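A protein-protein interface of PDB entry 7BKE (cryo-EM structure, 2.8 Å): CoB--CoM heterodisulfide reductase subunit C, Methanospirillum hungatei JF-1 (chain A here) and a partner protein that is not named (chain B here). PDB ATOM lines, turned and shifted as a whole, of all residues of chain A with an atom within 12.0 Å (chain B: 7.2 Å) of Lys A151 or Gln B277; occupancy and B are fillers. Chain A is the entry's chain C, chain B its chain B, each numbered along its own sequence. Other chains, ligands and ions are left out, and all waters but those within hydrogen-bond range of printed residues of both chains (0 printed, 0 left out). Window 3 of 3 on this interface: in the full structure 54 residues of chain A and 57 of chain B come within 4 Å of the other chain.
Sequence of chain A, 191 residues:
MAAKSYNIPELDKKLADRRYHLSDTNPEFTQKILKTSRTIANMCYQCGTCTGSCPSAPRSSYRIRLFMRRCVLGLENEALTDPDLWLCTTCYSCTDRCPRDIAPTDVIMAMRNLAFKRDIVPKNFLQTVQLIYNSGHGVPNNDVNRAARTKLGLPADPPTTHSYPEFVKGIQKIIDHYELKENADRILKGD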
ATOM      1  N   ASN A 141      37.482 -25.925 -13.860  1.00  0.00           N
ATOM      2  CA  ASN A 141      36.079 -26.308 -13.921  1.00  0.00           C
ATOM      3  C   ASN A 141      35.664 -27.054 -12.660  1.00  0.00           C
ATOM      4  O   ASN A 141      36.485 -27.680 -11.985  1.00  0.00           O
ATOM      5  CB  ASN A 141      35.832 -27.195 -15.140  1.00  0.00           C
ATOM      6  CG  ASN A 141      34.499 -26.933 -15.794  1.00  0.00           C
ATOM      7  OD1 ASN A 141      33.729 -26.096 -15.340  1.00  0.00           O
ATOM      8  ND2 ASN A 141      34.219 -27.654 -16.867  1.00  0.00           N
ATOM      9  N   ASN A 142      34.373 -26.994 -12.351  1.00  0.00           N
ATOM     10  CA  ASN A 142      33.802 -27.743 -11.242  1.00  0.00           C
ATOM     11  C   ASN A 142      32.524 -28.438 -11.702  1.00  0.00           C
ATOM     12  O   ASN A 142      32.093 -28.304 -12.849  1.00  0.00           O
ATOM     13  CB  ASN A 142      33.536 -26.835 -10.035  1.00  0.00           C
ATOM     14  CG  ASN A 142      32.895 -25.532 -10.423  1.00  0.00           C
ATOM     15  OD1 ASN A 142      32.374 -25.390 -11.525  1.00  0.00           O
ATOM     16  ND2 ASN A 142      32.926 -24.563  -9.517  1.00  0.00           N
ATOM     17  N   ASP A 143      31.916 -29.187 -10.781  1.00  0.00           N
ATOM     18  CA  ASP A 143      30.749 -29.996 -11.118  1.00  0.00           C
ATOM     19  C   ASP A 143      29.559 -29.137 -11.530  1.00  0.00           C
ATOM     20  O   ASP A 143      28.834 -29.478 -12.473  1.00  0.00           O
ATOM     21  CB  ASP A 143      30.384 -30.892  -9.934  1.00  0.00           C
ATOM     22  CG  ASP A 143      29.990 -30.098  -8.694  1.00  0.00           C
ATOM     23  OD1 ASP A 143      30.037 -28.850  -8.734  1.00  0.00           O
ATOM     24  OD2 ASP A 143      29.628 -30.723  -7.675  1.00  0.00           O
ATOM     25  N   VAL A 144      29.329 -28.029 -10.826  1.00  0.00           N
ATOM     26  CA  VAL A 144      28.166 -27.202 -11.128  1.00  0.00           C
ATOM     27  C   VAL A 144      28.313 -26.556 -12.498  1.00  0.00           C
ATOM     28  O   VAL A 144      27.341 -26.436 -13.252  1.00  0.00           O
ATOM     29  CB  VAL A 144      27.938 -26.159 -10.019  1.00  0.00           C
ATOM     30  CG1 VAL A 144      29.121 -25.216  -9.902  1.00  0.00           C
ATOM     31  CG2 VAL A 144      26.655 -25.388 -10.278  1.00  0.00           C
ATOM     32  N   ASN A 145      29.531 -26.152 -12.859  1.00  0.00           N
ATOM     33  CA  ASN A 145      29.724 -25.593 -14.186  1.00  0.00           C
ATOM     34  C   ASN A 145      29.657 -26.665 -15.260  1.00  0.00           C
ATOM     35  O   ASN A 145      29.212 -26.385 -16.372  1.00  0.00           O
ATOM     36  CB  ASN A 145      31.045 -24.845 -14.279  1.00  0.00           C
ATOM     37  CG  ASN A 145      31.071 -23.876 -15.428  1.00  0.00           C
ATOM     38  OD1 ASN A 145      30.564 -22.765 -15.322  1.00  0.00           O
ATOM     39  ND2 ASN A 145      31.645 -24.297 -16.543  1.00  0.00           N
ATOM     40  N   ARG A 146      30.096 -27.889 -14.959  1.00  0.00           N
ATOM     41  CA  ARG A 146      29.898 -28.974 -15.915  1.00  0.00           C
ATOM     42  C   ARG A 146      28.417 -29.195 -16.178  1.00  0.00           C
ATOM     43  O   ARG A 146      27.996 -29.351 -17.331  1.00  0.00           O
ATOM     44  CB  ARG A 146      30.550 -30.258 -15.406  1.00  0.00           C
ATOM     45  CG  ARG A 146      32.056 -30.232 -15.439  1.00  0.00           C
ATOM     46  CD  ARG A 146      32.651 -31.398 -14.687  1.00  0.00           C
ATOM     47  NE  ARG A 146      34.089 -31.481 -14.904  1.00  0.00           N
ATOM     48  CZ  ARG A 146      35.000 -31.064 -14.033  1.00  0.00           C
ATOM     49  NH1 ARG A 146      34.625 -30.541 -12.876  1.00  0.00           N
ATOM     50  NH2 ARG A 146      36.289 -31.174 -14.318  1.00  0.00           N
ATOM     51  N   ALA A 147      27.608 -29.185 -15.120  1.00  0.00           N
ATOM     52  CA  ALA A 147      26.164 -29.325 -15.290  1.00  0.00           C
ATOM     53  C   ALA A 147      25.583 -28.163 -16.089  1.00  0.00           C
ATOM     54  O   ALA A 147      24.718 -28.363 -16.949  1.00  0.00           O
ATOM     55  CB  ALA A 147      25.489 -29.429 -13.928  1.00  0.00           C
ATOM     56  N   ALA A 148      26.042 -26.939 -15.814  1.00  0.00           N
ATOM     57  CA  ALA A 148      25.548 -25.782 -16.552  1.00  0.00           C
ATOM     58  C   ALA A 148      25.904 -25.872 -18.032  1.00  0.00           C
ATOM     59  O   ALA A 148      25.070 -25.580 -18.896  1.00  0.00           O
ATOM     60  CB  ALA A 148      26.110 -24.499 -15.949  1.00  0.00           C
ATOM     61  N   ARG A 149      27.138 -26.265 -18.339  1.00  0.00           N
ATOM     62  CA  ARG A 149      27.545 -26.425 -19.729  1.00  0.00           C
ATOM     63  C   ARG A 149      26.709 -27.489 -20.420  1.00  0.00           C
ATOM     64  O   ARG A 149      26.287 -27.310 -21.570  1.00  0.00           O
ATOM     65  CB  ARG A 149      29.023 -26.786 -19.802  1.00  0.00           C
ATOM     66  CG  ARG A 149      29.945 -25.666 -19.415  1.00  0.00           C
ATOM     67  CD  ARG A 149      31.382 -26.106 -19.474  1.00  0.00           C
ATOM     68  NE  ARG A 149      31.701 -26.675 -20.771  1.00  0.00           N
ATOM     69  CZ  ARG A 149      32.281 -26.003 -21.754  1.00  0.00           C
ATOM     70  NH1 ARG A 149      32.602 -24.729 -21.590  1.00  0.00           N
ATOM     71  NH2 ARG A 149      32.536 -26.602 -22.903  1.00  0.00           N
ATOM     72  N   THR A 150      26.461 -28.605 -19.736  1.00  0.00           N
ATOM     73  CA  THR A 150      25.621 -29.647 -20.311  1.00  0.00           C
ATOM     74  C   THR A 150      24.219 -29.131 -20.602  1.00  0.00           C
ATOM     75  O   THR A 150      23.669 -29.381 -21.680  1.00  0.00           O
ATOM     76  CB  THR A 150      25.564 -30.847 -19.371  1.00  0.00           C
ATOM     77  OG1 THR A 150      26.885 -31.364 -19.176  1.00  0.00           O
ATOM     78  CG2 THR A 150      24.679 -31.930 -19.948  1.00  0.00           C
ATOM     79  N   LYS A 151      23.627 -28.396 -19.659  1.00  0.00           N
ATOM     80  CA  LYS A 151      22.282 -27.878 -19.893  1.00  0.00           C
ATOM     81  C   LYS A 151      22.273 -26.868 -21.033  1.00  0.00           C
ATOM     82  O   LYS A 151      21.280 -26.760 -21.759  1.00  0.00           O
ATOM     83  CB  LYS A 151      21.717 -27.269 -18.609  1.00  0.00           C
ATOM     84  CG  LYS A 151      20.299 -26.718 -18.727  1.00  0.00           C
ATOM     85  CD  LYS A 151      20.247 -25.233 -19.052  1.00  0.00           C
ATOM     86  CE  LYS A 151      20.699 -24.388 -17.878  1.00  0.00           C
ATOM     87  NZ  LYS A 151      20.637 -22.926 -18.183  1.00  0.00           N
ATOM     88  N   LEU A 152      23.365 -26.122 -21.201  1.00  0.00           N
ATOM     89  CA  LEU A 152      23.491 -25.243 -22.359  1.00  0.00           C
ATOM     90  C   LEU A 152      23.493 -26.045 -23.651  1.00  0.00           C
ATOM     91  O   LEU A 152      22.790 -25.707 -24.611  1.00  0.00           O
ATOM     92  CB  LEU A 152      24.773 -24.418 -22.258  1.00  0.00           C
ATOM     93  CG  LEU A 152      24.772 -23.173 -21.382  1.00  0.00           C
ATOM     94  CD1 LEU A 152      26.008 -22.349 -21.667  1.00  0.00           C
ATOM     95  CD2 LEU A 152      23.520 -22.373 -21.623  1.00  0.00           C
ATOM     96  N   GLY A 153      24.276 -27.115 -23.692  1.00  0.00           N
ATOM     97  CA  GLY A 153      24.491 -27.877 -24.907  1.00  0.00           C
ATOM     98  C   GLY A 153      25.946 -28.054 -25.271  1.00  0.00           C
ATOM     99  O   GLY A 153      26.253 -28.826 -26.188  1.00  0.00           O
ATOM    100  N   LEU A 154      26.853 -27.365 -24.592  1.00  0.00           N
ATOM    101  CA  LEU A 154      28.267 -27.580 -24.794  1.00  0.00           C
ATOM    102  C   LEU A 154      28.691 -28.908 -24.170  1.00  0.00           C
ATOM    103  O   LEU A 154      27.989 -29.458 -23.320  1.00  0.00           O
ATOM    104  CB  LEU A 154      29.064 -26.436 -24.174  1.00  0.00           C
ATOM    105  CG  LEU A 154      28.673 -25.032 -24.628  1.00  0.00           C
ATOM    106  CD1 LEU A 154      28.958 -24.032 -23.535  1.00  0.00           C
ATOM    107  CD2 LEU A 154      29.420 -24.676 -25.889  1.00  0.00           C
ATOM    108  N   PRO A 155      29.832 -29.451 -24.588  1.00  0.00           N
ATOM    109  CA  PRO A 155      30.384 -30.613 -23.890  1.00  0.00           C
ATOM    110  C   PRO A 155      30.680 -30.277 -22.437  1.00  0.00           C
ATOM    111  O   PRO A 155      30.954 -29.130 -22.088  1.00  0.00           O
ATOM    112  CB  PRO A 155      31.666 -30.926 -24.669  1.00  0.00           C
ATOM    113  CG  PRO A 155      31.903 -29.752 -25.548  1.00  0.00           C
ATOM    114  CD  PRO A 155      30.573 -29.157 -25.823  1.00  0.00           C
ATOM    115  N   ALA A 156      30.607 -31.301 -21.585  1.00  0.00           N
ATOM    116  CA  ALA A 156      30.745 -31.094 -20.150  1.00  0.00           C
ATOM    117  C   ALA A 156      32.096 -30.514 -19.775  1.00  0.00           C
ATOM    118  O   ALA A 156      32.235 -29.964 -18.680  1.00  0.00           O
ATOM    119  CB  ALA A 156      30.524 -32.406 -19.403  1.00  0.00           C
ATOM    120  N   ASP A 157      33.091 -30.629 -20.645  1.00  0.00           N
ATOM    121  CA  ASP A 157      34.381 -29.999 -20.435  1.00  0.00           C
ATOM    122  C   ASP A 157      34.805 -29.252 -21.688  1.00  0.00           C
ATOM    123  O   ASP A 157      34.500 -29.679 -22.805  1.00  0.00           O
ATOM    124  CB  ASP A 157      35.455 -31.027 -20.067  1.00  0.00           C
ATOM    125  CG  ASP A 157      35.454 -31.356 -18.597  1.00  0.00           C
ATOM    126  OD1 ASP A 157      35.103 -30.468 -17.795  1.00  0.00           O
ATOM    127  OD2 ASP A 157      35.804 -32.498 -18.242  1.00  0.00           O
ATOM    128  N   GLY B  18      27.950 -19.307 -21.018  1.00  0.00           N
ATOM    129  CA  GLY B  18      27.092 -18.632 -21.970  1.00  0.00           C
ATOM    130  C   GLY B  18      27.857 -17.658 -22.835  1.00  0.00           C
ATOM    131  O   GLY B  18      27.510 -17.452 -23.996  1.00  0.00           O
ATOM    132  N   MET B 274      18.947 -15.086 -29.161  1.00  0.00           N
ATOM    133  CA  MET B 274      19.216 -16.228 -28.302  1.00  0.00           C
ATOM    134  C   MET B 274      18.448 -16.089 -26.994  1.00  0.00           C
ATOM    135  O   MET B 274      18.111 -14.987 -26.560  1.00  0.00           O
ATOM    136  CB  MET B 274      20.711 -16.340 -28.032  1.00  0.00           C
ATOM    137  CG  MET B 274      21.510 -16.761 -29.248  1.00  0.00           C
ATOM    138  SD  MET B 274      23.195 -17.231 -28.847  1.00  0.00           S
ATOM    139  CE  MET B 274      22.891 -18.521 -27.649  1.00  0.00           C
ATOM    140  N   SER B 275      18.153 -17.216 -26.378  1.00  0.00           N
ATOM    141  CA  SER B 275      17.328 -17.173 -25.184  1.00  0.00           C
ATOM    142  C   SER B 275      18.183 -16.931 -23.946  1.00  0.00           C
ATOM    143  O   SER B 275      19.369 -17.267 -23.925  1.00  0.00           O
ATOM    144  CB  SER B 275      16.556 -18.477 -25.023  1.00  0.00           C
ATOM    145  OG  SER B 275      17.385 -19.512 -24.546  1.00  0.00           O
ATOM    146  N   PRO B 276      17.609 -16.331 -22.901  1.00  0.00           N
ATOM    147  CA  PRO B 276      18.366 -16.189 -21.648  1.00  0.00           C
ATOM    148  C   PRO B 276      18.823 -17.516 -21.069  1.00  0.00           C
ATOM    149  O   PRO B 276      19.929 -17.600 -20.521  1.00  0.00           O
ATOM    150  CB  PRO B 276      17.372 -15.472 -20.730  1.00  0.00           C
ATOM    151  CG  PRO B 276      16.485 -14.728 -21.665  1.00  0.00           C
ATOM    152  CD  PRO B 276      16.339 -15.593 -22.873  1.00  0.00           C
ATOM    153  N   GLN B 277      18.005 -18.563 -21.184  1.00  0.00           N
ATOM    154  CA  GLN B 277      18.447 -19.881 -20.747  1.00  0.00           C
ATOM    155  C   GLN B 277      19.611 -20.376 -21.595  1.00  0.00           C
ATOM    156  O   GLN B 277      20.555 -20.977 -21.072  1.00  0.00           O
ATOM    157  CB  GLN B 277      17.294 -20.884 -20.790  1.00  0.00           C
ATOM    158  CG  GLN B 277      16.173 -20.651 -19.782  1.00  0.00           C
ATOM    159  CD  GLN B 277      15.374 -19.397 -20.044  1.00  0.00           C
ATOM    160  OE1 GLN B 277      14.747 -19.250 -21.093  1.00  0.00           O
ATOM    161  NE2 GLN B 277      15.393 -18.476 -19.090  1.00  0.00           N
ATOM    162  N   ASP B 278      19.561 -20.139 -22.906  1.00  0.00           N
ATOM    163  CA  ASP B 278      20.658 -20.552 -23.771  1.00  0.00           C
ATOM    164  C   ASP B 278      21.909 -19.718 -23.550  1.00  0.00           C
ATOM    165  O   ASP B 278      22.992 -20.125 -23.978  1.00  0.00           O
ATOM    166  CB  ASP B 278      20.243 -20.463 -25.236  1.00  0.00           C
ATOM    167  CG  ASP B 278      19.199 -21.496 -25.608  1.00  0.00           C
ATOM    168  OD1 ASP B 278      19.178 -22.581 -24.986  1.00  0.00           O
ATOM    169  OD2 ASP B 278      18.393 -21.215 -26.519  1.00  0.00           O
ATOM    170  N   LEU B 279      21.776 -18.556 -22.922  1.00  0.00           N
ATOM    171  CA  LEU B 279      22.922 -17.740 -22.550  1.00  0.00           C
ATOM    172  C   LEU B 279      23.383 -17.985 -21.126  1.00  0.00           C
ATOM    173  O   LEU B 279      24.436 -17.471 -20.738  1.00  0.00           O
ATOM    174  CB  LEU B 279      22.591 -16.258 -22.724  1.00  0.00           C
ATOM    175  CG  LEU B 279      22.384 -15.847 -24.174  1.00  0.00           C
ATOM    176  CD1 LEU B 279      22.093 -14.376 -24.272  1.00  0.00           C
ATOM    177  CD2 LEU B 279      23.613 -16.198 -24.953  1.00  0.00           C
ATOM    178  N   ALA B 280      22.620 -18.744 -20.343  1.00  0.00           N
ATOM    179  CA  ALA B 280      22.984 -19.084 -18.972  1.00  0.00           C
ATOM    180  C   ALA B 280      23.162 -17.831 -18.122  1.00  0.00           C
ATOM    181  O   ALA B 280      24.127 -17.689 -17.371  1.00  0.00           O
ATOM    182  CB  ALA B 280      24.243 -19.956 -18.933  1.00  0.00           C
ATOM    183  N   LEU B 281      22.204 -16.912 -18.236  1.00  0.00           N
ATOM    184  CA  LEU B 281      22.231 -15.711 -17.417  1.00  0.00           C
ATOM    185  C   LEU B 281      21.936 -16.002 -15.954  1.00  0.00           C
ATOM    186  O   LEU B 281      22.082 -15.104 -15.119  1.00  0.00           O
ATOM    187  CB  LEU B 281      21.242 -14.682 -17.958  1.00  0.00           C
ATOM    188  CG  LEU B 281      21.432 -14.289 -19.423  1.00  0.00           C
ATOM    189  CD1 LEU B 281      20.595 -13.077 -19.750  1.00  0.00           C
ATOM    190  CD2 LEU B 281      22.885 -14.018 -19.716  1.00  0.00           C
ATOM    191  N   ASP B 282      21.523 -17.223 -15.627  1.00  0.00           N
ATOM    192  CA  ASP B 282      21.320 -17.633 -14.246  1.00  0.00           C
ATOM    193  C   ASP B 282      22.623 -17.912 -13.518  1.00  0.00           C
ATOM    194  O   ASP B 282      22.601 -18.112 -12.300  1.00  0.00           O
ATOM    195  CB  ASP B 282      20.441 -18.878 -14.205  1.00  0.00           C
ATOM    196  CG  ASP B 282      19.073 -18.637 -14.789  1.00  0.00           C
ATOM    197  OD1 ASP B 282      18.564 -17.505 -14.655  1.00  0.00           O
ATOM    198  OD2 ASP B 282      18.512 -19.572 -15.399  1.00  0.00           O
ATOM    199  N   LEU B 283      23.747 -17.944 -14.228  1.00  0.00           N
ATOM    200  CA  LEU B 283      25.047 -18.200 -13.627  1.00  0.00           C
ATOM    201  C   LEU B 283      25.749 -16.933 -13.160  1.00  0.00           C
ATOM    202  O   LEU B 283      26.859 -17.021 -12.624  1.00  0.00           O
ATOM    203  CB  LEU B 283      25.944 -18.946 -14.616  1.00  0.00           C
ATOM    204  CG  LEU B 283      26.049 -20.453 -14.386  1.00  0.00           C
ATOM    205  CD1 LEU B 283      24.694 -21.123 -14.527  1.00  0.00           C
ATOM    206  CD2 LEU B 283      27.046 -21.059 -15.343  1.00  0.00           C
ATOM    207  N   LEU B 292      16.350  -7.628 -18.601  1.00  0.00           N
ATOM    208  CA  LEU B 292      15.565  -8.424 -19.535  1.00  0.00           C
ATOM    209  C   LEU B 292      14.140  -7.905 -19.658  1.00  0.00           C
ATOM    210  O   LEU B 292      13.572  -7.907 -20.754  1.00  0.00           O
ATOM    211  CB  LEU B 292      15.586  -9.889 -19.116  1.00  0.00           C
ATOM    212  CG  LEU B 292      16.760 -10.705 -19.654  1.00  0.00           C
ATOM    213  CD1 LEU B 292      18.077 -10.227 -19.127  1.00  0.00           C
ATOM    214  CD2 LEU B 292      16.563 -12.136 -19.232  1.00  0.00           C
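O of Gln B277 is in hydrogen-bond range of NZ of Lys A151 (3.5 Å).
The side-chain amide oxygen (OD1) of Asn A141 lies within hydrogen-bond range of the side-chain amide nitrogen (ND2) of Asn A145, 3.0 Å away.
The backbone NH of Asn A145 sits close to the side-chain amide oxygen of Asn A142 (3.2 Å).
The side-chain hydroxyl (OG) of Ser B275 lies within hydrogen-bond range of the side-chain carboxylate (OD2) of Asp B278, at 2.8 Å.
Among the printed residues, pairs that only touch across the chains: Asn A145 with Leu B283 (3.9 Å), Ala A148 with Leu B283 (3.6 Å), Leu A152 with Gly B18 (3.7 Å), Leu A152 with Gln B277 (3.3 Å), Leu A152 with Asp B278 (3.3 Å) and Leu A152 with Ala B280 (3.7 Å).
Printed residues of chain B within 4 Å of Lys A151: Gln B277.
Of chain A, only Lys A151 (3.5 Å) and Leu A152 (3.3 Å) come within 4 Å of Gln B277.
No residue of chain A comes within 4 Å of Ser B275.
No residue of chain A comes within 4 Å of Pro B276.
Of chain A, only Leu A152 comes within 4 Å of Asp B278.
Ala B280 touches just one residue of chain A: Leu A152.
No residue of chain A comes within 4 Å of Asp B282.
Of the printed residues of chain B, Asn A145 touches Leu B283.
Printed residues of chain A within 4 Å of Gly B18: Leu A152.
Of the printed residues of chain A, Leu B283 touches Asn A145 (3.9 Å) and Ala A148 (3.6 Å).
Of the printed residues of chain B, Ala A148 touches Leu B283 (3.6 Å).
Arg A146 touches none of the printed residues of chain B.
Leu B292 touches none of the printed residues of chain A.
The nearest residue of chain B that does not touch Lys A151 is Ala B280 (4.6 Å).
The nearest printed residue of chain A that does not touch Gly B18 is Leu A154 (5.4 Å).
Of the 12 printed residues of chain B, 5 touch a printed residue of chain A.
Printed residues of chain B that touch a printed residue of chain A: Gly B18, Gln B277, Asp B278, Ala B280 and Leu B283.
Hydrophobic or aromatic side chains of chain B that line the printed part of chain A: Ala B280 and Leu B283.
Of the 17 printed residues of chain A, 4 touch a printed residue of chain B.
Printed residues of chain A that touch a printed residue of chain B: Asn A145, Ala A148, Lys A151 and Leu A152.
Hydrophobic or aromatic side chains of chain A that line the printed part of chain B: Ala A148 and Leu A152.
Among the printed residues, 7 pairs touch across the chains.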
